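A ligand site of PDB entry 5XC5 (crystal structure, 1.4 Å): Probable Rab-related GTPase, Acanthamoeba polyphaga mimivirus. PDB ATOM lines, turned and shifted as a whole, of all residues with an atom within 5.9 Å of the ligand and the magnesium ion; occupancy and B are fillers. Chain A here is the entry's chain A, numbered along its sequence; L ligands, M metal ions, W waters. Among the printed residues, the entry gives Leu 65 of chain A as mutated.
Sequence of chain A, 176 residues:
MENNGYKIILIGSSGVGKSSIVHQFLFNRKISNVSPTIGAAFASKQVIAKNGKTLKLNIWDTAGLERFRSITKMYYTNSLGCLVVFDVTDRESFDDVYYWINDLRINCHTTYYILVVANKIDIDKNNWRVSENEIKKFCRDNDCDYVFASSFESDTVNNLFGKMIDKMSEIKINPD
Two residues have an atom within 4 Å of the magnesium ion: Ser 19 and Thr 37. The nearest printed residue that does not touch the magnesium ion is Asp 61 (4.05 Å).
N of Gly 64 sits at hydrogen-bond distance from O3 of the ligand (2.9 Å). N of Val 16 lies within hydrogen-bond range of O6 of the ligand (3.3 Å). The backbone NH (N) of Ser 20 sits at hydrogen-bond distance from an oxygen (O8) of the ligand, 2.8 Å away. The side-chain hydroxyl (OG) of Ser 151 is in hydrogen-bond range of a nitrogen (N2) of the ligand (2.6 Å). The side-chain hydroxyl (OG) of Ser 14 is in hydrogen-bond range of an oxygen (O2) of the ligand (2.8 Å). O1 of the ligand lies close to N of Thr 37, at 2.8 Å. The backbone NH of Ser 151 lies within hydrogen-bond range of an oxygen (O14) of the ligand (2.8 Å). NZ of Lys 18 lies within salt-bridge range of O3 of the ligand, 2.7 Å away. O6 of the ligand sits at hydrogen-bond distance from N of Gly 17 (3.0 Å). The backbone NH of Gly 15 sits at hydrogen-bond distance from an oxygen (O4) of the ligand (3.0 Å). OG of Ser 20 is in hydrogen-bond range of O8 of the ligand. An oxygen (O8) of the ligand is in hydrogen-bond range of the backbone NH (N) of Ser 19 (3.4 Å). An oxygen (O11) of the ligand sits at hydrogen-bond distance from the side-chain amino group (NZ) of Lys 120 (3.2 Å). The side-chain hydroxyl (OG) of Ser 150 sits at hydrogen-bond distance from an oxygen (O14) of the ligand. The backbone NH (N) of Lys 18 is in hydrogen-bond range of an oxygen (O6) of the ligand. OD1 of Asp 122 lies within hydrogen-bond range of N3 of the ligand (2.7 Å).
Residues that only touch the ligand: Val 34 (3.0 Å), Phe 152 (3.3 Å), Asn 119 (3.7 Å), Pro 36 (3.7 Å), Ile 123 (3.8 Å), Ser 13 (3.96 Å) and Ala 63 (3.97 Å). 20 residues have an atom within 4 Å of the ligand: Ser 13, Ser 14, Gly 15, Val 16, Gly 17, Lys 18, Ser 19, Ser 20, Val 34, Pro 36, Thr 37, Ala 63, Gly 64, Asn 119, Lys 120, Asp 122, Ile 123, Ser 150, Ser 151 and Phe 152.
Water W6 bridges O of Ser 35 (2.7 Å) and O9 of the ligand (2.7 Å). Water W3 bridges the side-chain carboxylate of Asp 61 (2.6 Å) and the backbone carbonyl oxygen of Thr 62 (2.7 Å). Water W4 bridges O13 of the ligand (2.8 Å) and OG of Ser 20 (2.8 Å). Water W5 lies within hydrogen-bond range of O of Thr 37 (2.7 Å), O2 of the ligand (2.9 Å), N of Leu 65 (3.0 Å) and N of Gly 64 (3.1 Å). Water W8 lies within hydrogen-bond range of NZ of Lys 120 (2.9 Å) and N5 of the ligand (2.9 Å).
The magnesium ion is bound by an oxygen (O1) of the ligand (2.0 Å), an oxygen (O5) of the ligand (2.0 Å), the side-chain hydroxyl (OG) of Ser 19 (2.1 Å), water W6 (2.1 Å), the side-chain hydroxyl (OG1) of Thr 37 (2.1 Å) and water W3 (2.2 Å).
The side-chain amide nitrogen (ND2) of Asn 119 sits at hydrogen-bond distance from the side-chain hydroxyl (OG) of Ser 151, at 3.1 Å. O of Ala 149 lies within hydrogen-bond range of N of Lys 120 (3.0 Å). The side-chain hydroxyl (OG) of Ser 150 lies within hydrogen-bond range of the side-chain carboxylate (OD1) of Asp 122 (2.9 Å). The backbone carbonyl oxygen (O) of Gly 12 lies within hydrogen-bond range of the side-chain amino group (NZ) of Lys 18 (2.9 Å). The side-chain amino group of Lys 120 sits at hydrogen-bond distance from the backbone carbonyl oxygen of Gly 15. The side-chain amino group (NZ) of Lys 18 sits at hydrogen-bond distance from the backbone carbonyl oxygen (O) of Ser 13 (3.0 Å). The side-chain amide nitrogen (ND2) of Asn 119 sits at hydrogen-bond distance from the backbone carbonyl oxygen (O) of Val 16 (2.9 Å). OG of Ser 150 sits close to N of Phe 152.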
ATOM      1  N   GLY A  12     -17.785 -27.305  -0.119  1.00  0.00           N
ATOM      2  CA  GLY A  12     -17.307 -27.890   1.125  1.00  0.00           C
ATOM      3  C   GLY A  12     -17.728 -29.334   1.206  1.00  0.00           C
ATOM      4  O   GLY A  12     -18.566 -29.812   0.453  1.00  0.00           O
ATOM      5  N   SER A  13     -17.095 -30.065   2.128  1.00  0.00           N
ATOM      6  CA  SER A  13     -17.268 -31.507   2.165  1.00  0.00           C
ATOM      7  C   SER A  13     -18.673 -31.864   2.648  1.00  0.00           C
ATOM      8  O   SER A  13     -19.417 -31.034   3.159  1.00  0.00           O
ATOM      9  CB  SER A  13     -16.186 -32.132   3.021  1.00  0.00           C
ATOM     10  OG  SER A  13     -14.944 -31.907   2.364  1.00  0.00           O
ATOM     11  N   SER A  14     -19.038 -33.130   2.448  1.00  0.00           N
ATOM     12  CA  SER A  14     -20.408 -33.540   2.726  1.00  0.00           C
ATOM     13  C   SER A  14     -20.703 -33.461   4.216  1.00  0.00           C
ATOM     14  O   SER A  14     -19.862 -33.810   5.051  1.00  0.00           O
ATOM     15  CB  SER A  14     -20.653 -34.961   2.224  1.00  0.00           C
ATOM     16  OG  SER A  14     -21.966 -35.374   2.544  1.00  0.00           O
ATOM     17  N   GLY A  15     -21.891 -32.972   4.547  1.00  0.00           N
ATOM     18  CA  GLY A  15     -22.356 -32.951   5.919  1.00  0.00           C
ATOM     19  C   GLY A  15     -22.004 -31.728   6.716  1.00  0.00           C
ATOM     20  O   GLY A  15     -22.423 -31.628   7.877  1.00  0.00           O
ATOM     21  N   VAL A  16     -21.285 -30.768   6.125  1.00  0.00           N
ATOM     22  CA  VAL A  16     -20.800 -29.613   6.901  1.00  0.00           C
ATOM     23  C   VAL A  16     -21.891 -28.582   7.155  1.00  0.00           C
ATOM     24  O   VAL A  16     -21.689 -27.699   8.004  1.00  0.00           O
ATOM     25  CB  VAL A  16     -19.570 -28.947   6.252  1.00  0.00           C
ATOM     26  CG1 VAL A  16     -18.410 -29.937   6.159  1.00  0.00           C
ATOM     27  CG2 VAL A  16     -19.906 -28.375   4.887  1.00  0.00           C
ATOM     28  N   GLY A  17     -23.018 -28.656   6.456  1.00  0.00           N
ATOM     29  CA  GLY A  17     -24.125 -27.758   6.639  1.00  0.00           C
ATOM     30  C   GLY A  17     -24.353 -26.696   5.553  1.00  0.00           C
ATOM     31  O   GLY A  17     -25.056 -25.724   5.827  1.00  0.00           O
ATOM     32  N   LYS A  18     -23.802 -26.891   4.340  1.00  0.00           N
ATOM     33  CA  LYS A  18     -24.025 -25.921   3.266  1.00  0.00           C
ATOM     34  C   LYS A  18     -25.518 -25.712   3.000  1.00  0.00           C
ATOM     35  O   LYS A  18     -25.995 -24.577   2.938  1.00  0.00           O
ATOM     36  CB  LYS A  18     -23.316 -26.396   2.000  1.00  0.00           C
ATOM     37  CG  LYS A  18     -21.807 -26.528   2.137  1.00  0.00           C
ATOM     38  CD  LYS A  18     -21.163 -27.050   0.846  1.00  0.00           C
ATOM     39  CE  LYS A  18     -21.691 -28.423   0.436  1.00  0.00           C
ATOM     40  NZ  LYS A  18     -21.313 -29.529   1.376  1.00  0.00           N
ATOM     41  N   SER A  19     -26.254 -26.808   2.803  1.00  0.00           N
ATOM     42  CA  SER A  19     -27.669 -26.671   2.466  1.00  0.00           C
ATOM     43  C   SER A  19     -28.467 -26.093   3.620  1.00  0.00           C
ATOM     44  O   SER A  19     -29.396 -25.295   3.415  1.00  0.00           O
ATOM     45  CB  SER A  19     -28.253 -28.016   2.021  1.00  0.00           C
ATOM     46  OG  SER A  19     -27.582 -28.520   0.884  1.00  0.00           O
ATOM     47  N   SER A  20     -28.119 -26.473   4.851  1.00  0.00           N
ATOM     48  CA  SER A  20     -28.797 -25.914   6.020  1.00  0.00           C
ATOM     49  C   SER A  20     -28.581 -24.416   6.117  1.00  0.00           C
ATOM     50  O   SER A  20     -29.522 -23.658   6.403  1.00  0.00           O
ATOM     51  CB  SER A  20     -28.293 -26.621   7.275  1.00  0.00           C
ATOM     52  OG  SER A  20     -28.620 -27.996   7.232  1.00  0.00           O
ATOM     53  N   ILE A  21     -27.359 -23.950   5.846  1.00  0.00           N
ATOM     54  CA  ILE A  21     -27.067 -22.521   5.831  1.00  0.00           C
ATOM     55  C   ILE A  21     -27.897 -21.809   4.770  1.00  0.00           C
ATOM     56  O   ILE A  21     -28.528 -20.776   5.031  1.00  0.00           O
ATOM     57  CB  ILE A  21     -25.560 -22.294   5.627  1.00  0.00           C
ATOM     58  CG1 ILE A  21     -24.808 -22.578   6.930  1.00  0.00           C
ATOM     59  CG2 ILE A  21     -25.292 -20.885   5.146  1.00  0.00           C
ATOM     60  CD1 ILE A  21     -23.295 -22.733   6.733  1.00  0.00           C
ATOM     61  N   VAL A  34     -33.887 -31.336   4.612  1.00  0.00           N
ATOM     62  CA  VAL A  34     -32.518 -31.382   4.089  1.00  0.00           C
ATOM     63  C   VAL A  34     -32.060 -32.826   3.914  1.00  0.00           C
ATOM     64  O   VAL A  34     -32.121 -33.627   4.861  1.00  0.00           O
ATOM     65  CB  VAL A  34     -31.526 -30.584   4.952  1.00  0.00           C
ATOM     66  CG1 VAL A  34     -30.176 -30.589   4.290  1.00  0.00           C
ATOM     67  CG2 VAL A  34     -32.006 -29.151   5.123  1.00  0.00           C
ATOM     68  N   SER A  35     -31.568 -33.145   2.728  1.00  0.00           N
ATOM     69  CA  SER A  35     -30.955 -34.412   2.363  1.00  0.00           C
ATOM     70  C   SER A  35     -29.703 -34.095   1.563  1.00  0.00           C
ATOM     71  O   SER A  35     -29.533 -32.968   1.085  1.00  0.00           O
ATOM     72  CB  SER A  35     -31.927 -35.239   1.499  1.00  0.00           C
ATOM     73  OG  SER A  35     -32.395 -34.479   0.408  1.00  0.00           O
ATOM     74  N   PRO A  36     -28.775 -35.061   1.414  1.00  0.00           N
ATOM     75  CA  PRO A  36     -27.517 -34.770   0.727  1.00  0.00           C
ATOM     76  C   PRO A  36     -27.733 -34.228  -0.680  1.00  0.00           C
ATOM     77  O   PRO A  36     -28.592 -34.694  -1.430  1.00  0.00           O
ATOM     78  CB  PRO A  36     -26.782 -36.121   0.706  1.00  0.00           C
ATOM     79  CG  PRO A  36     -27.375 -36.878   1.830  1.00  0.00           C
ATOM     80  CD  PRO A  36     -28.795 -36.435   1.954  1.00  0.00           C
ATOM     81  N   THR A  37     -26.951 -33.219  -1.025  1.00  0.00           N
ATOM     82  CA  THR A  37     -27.073 -32.571  -2.313  1.00  0.00           C
ATOM     83  C   THR A  37     -26.338 -33.383  -3.375  1.00  0.00           C
ATOM     84  O   THR A  37     -25.242 -33.909  -3.138  1.00  0.00           O
ATOM     85  CB  THR A  37     -26.506 -31.162  -2.222  1.00  0.00           C
ATOM     86  OG1 THR A  37     -27.118 -30.497  -1.090  1.00  0.00           O
ATOM     87  CG2 THR A  37     -26.781 -30.353  -3.500  1.00  0.00           C
ATOM     88  N   ILE A  38     -26.960 -33.507  -4.545  1.00  0.00           N
ATOM     89  CA  ILE A  38     -26.327 -34.184  -5.680  1.00  0.00           C
ATOM     90  C   ILE A  38     -26.097 -33.144  -6.765  1.00  0.00           C
ATOM     91  O   ILE A  38     -25.063 -32.448  -6.758  1.00  0.00           O
ATOM     92  CB  ILE A  38     -27.141 -35.393  -6.158  1.00  0.00           C
ATOM     93  CG1 ILE A  38     -27.455 -36.301  -4.962  1.00  0.00           C
ATOM     94  CG2 ILE A  38     -26.356 -36.173  -7.234  1.00  0.00           C
ATOM     95  CD1 ILE A  38     -28.152 -37.614  -5.329  1.00  0.00           C
ATOM     96  N   ASP A  61     -25.987 -24.133  -4.449  1.00  0.00           N
ATOM     97  CA  ASP A  61     -25.649 -25.004  -3.341  1.00  0.00           C
ATOM     98  C   ASP A  61     -25.191 -26.333  -3.939  1.00  0.00           C
ATOM     99  O   ASP A  61     -25.963 -26.999  -4.627  1.00  0.00           O
ATOM    100  CB  ASP A  61     -26.920 -25.207  -2.506  1.00  0.00           C
ATOM    101  CG  ASP A  61     -26.732 -26.152  -1.348  1.00  0.00           C
ATOM    102  OD1 ASP A  61     -25.566 -26.352  -0.929  1.00  0.00           O
ATOM    103  OD2 ASP A  61     -27.753 -26.702  -0.851  1.00  0.00           O
ATOM    104  N   THR A  62     -23.928 -26.696  -3.711  1.00  0.00           N
ATOM    105  CA  THR A  62     -23.315 -27.813  -4.436  1.00  0.00           C
ATOM    106  C   THR A  62     -23.103 -29.029  -3.534  1.00  0.00           C
ATOM    107  O   THR A  62     -23.190 -28.955  -2.316  1.00  0.00           O
ATOM    108  CB  THR A  62     -21.971 -27.404  -5.067  1.00  0.00           C
ATOM    109  OG1 THR A  62     -21.000 -27.188  -4.029  1.00  0.00           O
ATOM    110  CG2 THR A  62     -22.099 -26.142  -5.890  1.00  0.00           C
ATOM    111  N   ALA A  63     -22.810 -30.156  -4.183  1.00  0.00           N
ATOM    112  CA  ALA A  63     -22.567 -31.413  -3.483  1.00  0.00           C
ATOM    113  C   ALA A  63     -21.174 -31.463  -2.878  1.00  0.00           C
ATOM    114  O   ALA A  63     -20.178 -31.140  -3.524  1.00  0.00           O
ATOM    115  CB  ALA A  63     -22.696 -32.570  -4.468  1.00  0.00           C
ATOM    116  N   GLY A  64     -21.104 -31.947  -1.637  1.00  0.00           N
ATOM    117  CA  GLY A  64     -19.843 -32.251  -0.987  1.00  0.00           C
ATOM    118  C   GLY A  64     -19.414 -33.709  -1.047  1.00  0.00           C
ATOM    119  O   GLY A  64     -18.249 -34.002  -0.784  1.00  0.00           O
ATOM    120  N   LEU A  65     -20.336 -34.615  -1.387  1.00  0.00           N
ATOM    121  CA  LEU A  65     -19.977 -36.027  -1.484  1.00  0.00           C
ATOM    122  C   LEU A  65     -18.917 -36.234  -2.561  1.00  0.00           C
ATOM    123  O   LEU A  65     -19.016 -35.692  -3.668  1.00  0.00           O
ATOM    124  CB  LEU A  65     -21.202 -36.872  -1.795  1.00  0.00           C
ATOM    125  CG  LEU A  65     -22.137 -37.099  -0.603  1.00  0.00           C
ATOM    126  CD1 LEU A  65     -23.445 -37.640  -1.117  1.00  0.00           C
ATOM    127  CD2 LEU A  65     -21.538 -38.052   0.427  1.00  0.00           C
ATOM    128  N   ASN A 119     -18.525 -23.850  10.595  1.00  0.00           N
ATOM    129  CA  ASN A 119     -19.913 -24.110  10.929  1.00  0.00           C
ATOM    130  C   ASN A 119     -20.023 -25.107  12.081  1.00  0.00           C
ATOM    131  O   ASN A 119     -19.079 -25.811  12.442  1.00  0.00           O
ATOM    132  CB  ASN A 119     -20.676 -24.635   9.706  1.00  0.00           C
ATOM    133  CG  ASN A 119     -22.173 -24.442   9.818  1.00  0.00           C
ATOM    134  OD1 ASN A 119     -22.633 -23.520  10.471  1.00  0.00           O
ATOM    135  ND2 ASN A 119     -22.943 -25.318   9.177  1.00  0.00           N
ATOM    136  N   LYS A 120     -21.238 -25.155  12.629  1.00  0.00           N
ATOM    137  CA  LYS A 120     -21.628 -26.027  13.744  1.00  0.00           C
ATOM    138  C   LYS A 120     -21.058 -25.568  15.090  1.00  0.00           C
ATOM    139  O   LYS A 120     -20.829 -26.374  15.987  1.00  0.00           O
ATOM    140  CB  LYS A 120     -21.382 -27.525  13.498  1.00  0.00           C
ATOM    141  CG  LYS A 120     -21.875 -27.987  12.140  1.00  0.00           C
ATOM    142  CD  LYS A 120     -22.069 -29.476  12.087  1.00  0.00           C
ATOM    143  CE  LYS A 120     -22.441 -29.956  10.678  1.00  0.00           C
ATOM    144  NZ  LYS A 120     -22.622 -31.444  10.650  1.00  0.00           N
ATOM    145  N   ILE A 121     -20.861 -24.251  15.236  1.00  0.00           N
ATOM    146  CA  ILE A 121     -20.302 -23.714  16.477  1.00  0.00           C
ATOM    147  C   ILE A 121     -21.189 -23.969  17.693  1.00  0.00           C
ATOM    148  O   ILE A 121     -20.729 -23.793  18.820  1.00  0.00           O
ATOM    149  CB  ILE A 121     -19.936 -22.216  16.326  1.00  0.00           C
ATOM    150  CG1 ILE A 121     -21.203 -21.360  16.180  1.00  0.00           C
ATOM    151  CG2 ILE A 121     -18.945 -22.031  15.196  1.00  0.00           C
ATOM    152  CD1 ILE A 121     -20.922 -19.873  15.947  1.00  0.00           C
ATOM    153  N   ASP A 122     -22.454 -24.346  17.485  1.00  0.00           N
ATOM    154  CA  ASP A 122     -23.328 -24.692  18.593  1.00  0.00           C
ATOM    155  C   ASP A 122     -22.831 -25.909  19.350  1.00  0.00           C
ATOM    156  O   ASP A 122     -23.149 -26.058  20.536  1.00  0.00           O
ATOM    157  CB  ASP A 122     -24.750 -24.958  18.084  1.00  0.00           C
ATOM    158  CG  ASP A 122     -24.778 -26.033  17.002  1.00  0.00           C
ATOM    159  OD1 ASP A 122     -24.322 -25.737  15.875  1.00  0.00           O
ATOM    160  OD2 ASP A 122     -25.229 -27.159  17.273  1.00  0.00           O
ATOM    161  N   ILE A 123     -22.058 -26.787  18.696  1.00  0.00           N
ATOM    162  CA  ILE A 123     -21.546 -27.971  19.360  1.00  0.00           C
ATOM    163  C   ILE A 123     -20.578 -27.548  20.458  1.00  0.00           C
ATOM    164  O   ILE A 123     -19.820 -26.580  20.318  1.00  0.00           O
ATOM    165  CB  ILE A 123     -20.869 -28.879  18.314  1.00  0.00           C
ATOM    166  CG1 ILE A 123     -21.904 -29.380  17.308  1.00  0.00           C
ATOM    167  CG2 ILE A 123     -20.123 -30.044  18.999  1.00  0.00           C
ATOM    168  CD1 ILE A 123     -21.351 -30.184  16.162  1.00  0.00           C
ATOM    169  N   ALA A 149     -20.215 -19.811  12.362  1.00  0.00           N
ATOM    170  CA  ALA A 149     -21.665 -19.878  12.222  1.00  0.00           C
ATOM    171  C   ALA A 149     -22.243 -21.187  12.765  1.00  0.00           C
ATOM    172  O   ALA A 149     -21.524 -22.154  13.036  1.00  0.00           O
ATOM    173  CB  ALA A 149     -22.079 -19.701  10.758  1.00  0.00           C
ATOM    174  N   SER A 150     -23.567 -21.165  12.954  1.00  0.00           N
ATOM    175  CA  SER A 150     -24.379 -22.355  13.125  1.00  0.00           C
ATOM    176  C   SER A 150     -25.605 -22.187  12.238  1.00  0.00           C
ATOM    177  O   SER A 150     -26.262 -21.142  12.293  1.00  0.00           O
ATOM    178  CB  SER A 150     -24.848 -22.490  14.575  1.00  0.00           C
ATOM    179  OG  SER A 150     -25.827 -23.519  14.691  1.00  0.00           O
ATOM    180  N   SER A 151     -25.903 -23.210  11.428  1.00  0.00           N
ATOM    181  CA  SER A 151     -27.061 -23.171  10.543  1.00  0.00           C
ATOM    182  C   SER A 151     -28.342 -22.894  11.301  1.00  0.00           C
ATOM    183  O   SER A 151     -29.286 -22.323  10.738  1.00  0.00           O
ATOM    184  CB  SER A 151     -27.224 -24.497   9.817  1.00  0.00           C
ATOM    185  OG  SER A 151     -26.018 -24.935   9.195  1.00  0.00           O
ATOM    186  N   PHE A 152     -28.412 -23.320  12.561  1.00  0.00           N
ATOM    187  CA  PHE A 152     -29.620 -23.220  13.363  1.00  0.00           C
ATOM    188  C   PHE A 152     -29.774 -21.869  14.032  1.00  0.00           C
ATOM    189  O   PHE A 152     -30.800 -21.614  14.662  1.00  0.00           O
ATOM    190  CB  PHE A 152     -29.633 -24.331  14.427  1.00  0.00           C
ATOM    191  CG  PHE A 152     -29.403 -25.709  13.872  1.00  0.00           C
ATOM    192  CD1 PHE A 152     -29.894 -26.046  12.618  1.00  0.00           C
ATOM    193  CD2 PHE A 152     -28.687 -26.651  14.591  1.00  0.00           C
ATOM    194  CE1 PHE A 152     -29.668 -27.301  12.090  1.00  0.00           C
ATOM    195  CE2 PHE A 152     -28.476 -27.922  14.064  1.00  0.00           C
ATOM    196  CZ  PHE A 152     -28.960 -28.247  12.814  1.00  0.00           C
HETATM  197  P1  LIG L   1     -23.925 -32.285   1.337  1.00  0.00           P
HETATM  198  O1  LIG L   1     -25.087 -31.747   0.517  1.00  0.00           O
HETATM  199  O2  LIG L   1     -23.973 -33.779   1.469  1.00  0.00           O
HETATM  200  O3  LIG L   1     -22.580 -31.802   0.815  1.00  0.00           O
HETATM  201  O4  LIG L   1     -24.049 -31.781   2.887  1.00  0.00           O
HETATM  202  P2  LIG L   1     -24.347 -30.276   3.415  1.00  0.00           P
HETATM  203  O5  LIG L   1     -25.342 -29.571   2.504  1.00  0.00           O
HETATM  204  O6  LIG L   1     -23.052 -29.530   3.612  1.00  0.00           O
HETATM  205  O7  LIG L   1     -24.910 -30.486   4.915  1.00  0.00           O
HETATM  206  P3  LIG L   1     -26.476 -30.443   5.363  1.00  0.00           P
HETATM  207  O8  LIG L   1     -27.004 -29.002   5.333  1.00  0.00           O
HETATM  208  O9  LIG L   1     -27.277 -31.495   4.556  1.00  0.00           O
HETATM  209  O10 LIG L   1     -26.337 -30.867   6.919  1.00  0.00           O
HETATM  210  C1  LIG L   1     -25.845 -32.132   7.299  1.00  0.00           C
HETATM  211  C2  LIG L   1     -26.311 -32.450   8.719  1.00  0.00           C
HETATM  212  O11 LIG L   1     -25.670 -31.539   9.594  1.00  0.00           O
HETATM  213  C3  LIG L   1     -27.802 -32.301   8.921  1.00  0.00           C
HETATM  214  O12 LIG L   1     -28.277 -33.325   9.785  1.00  0.00           O
HETATM  215  C4  LIG L   1     -27.928 -30.965   9.615  1.00  0.00           C
HETATM  216  O13 LIG L   1     -29.072 -30.877  10.439  1.00  0.00           O
HETATM  217  C5  LIG L   1     -26.639 -30.888  10.401  1.00  0.00           C
HETATM  218  N1  LIG L   1     -26.257 -29.484  10.590  1.00  0.00           N
HETATM  219  C6  LIG L   1     -26.226 -28.479   9.654  1.00  0.00           C
HETATM  220  N2  LIG L   1     -25.811 -27.339  10.233  1.00  0.00           N
HETATM  221  C7  LIG L   1     -25.581 -27.600  11.547  1.00  0.00           C
HETATM  222  C8  LIG L   1     -25.143 -26.809  12.603  1.00  0.00           C
HETATM  223  O14 LIG L   1     -24.868 -25.601  12.500  1.00  0.00           O
HETATM  224  N3  LIG L   1     -25.019 -27.416  13.831  1.00  0.00           N
HETATM  225  C9  LIG L   1     -25.290 -28.755  14.031  1.00  0.00           C
HETATM  226  N4  LIG L   1     -25.149 -29.259  15.250  1.00  0.00           N
HETATM  227  N5  LIG L   1     -25.715 -29.551  12.992  1.00  0.00           N
HETATM  228  C10 LIG L   1     -25.853 -28.948  11.781  1.00  0.00           C
HETATM  229 MG    MG M   1     -26.249 -30.096   0.759  1.00  0.00          MG
HETATM  230  O   HOH W   1     -25.372 -32.034  15.963  1.00  0.00           O
HETATM  231  O   HOH W   2     -29.003 -32.333  13.282  1.00  0.00           O
HETATM  232  O   HOH W   3     -24.875 -28.786  -0.262  1.00  0.00           O
HETATM  233  O   HOH W   4     -30.585 -29.249   8.772  1.00  0.00           O
HETATM  234  O   HOH W   5     -23.276 -34.117  -1.283  1.00  0.00           O
HETATM  235  O   HOH W   6     -27.620 -31.201   1.870  1.00  0.00           O
HETATM  236  O   HOH W   7     -26.817 -33.752  12.286  1.00  0.00           O
HETATM  237  O   HOH W   8     -24.496 -32.203  12.715  1.00  0.00           O
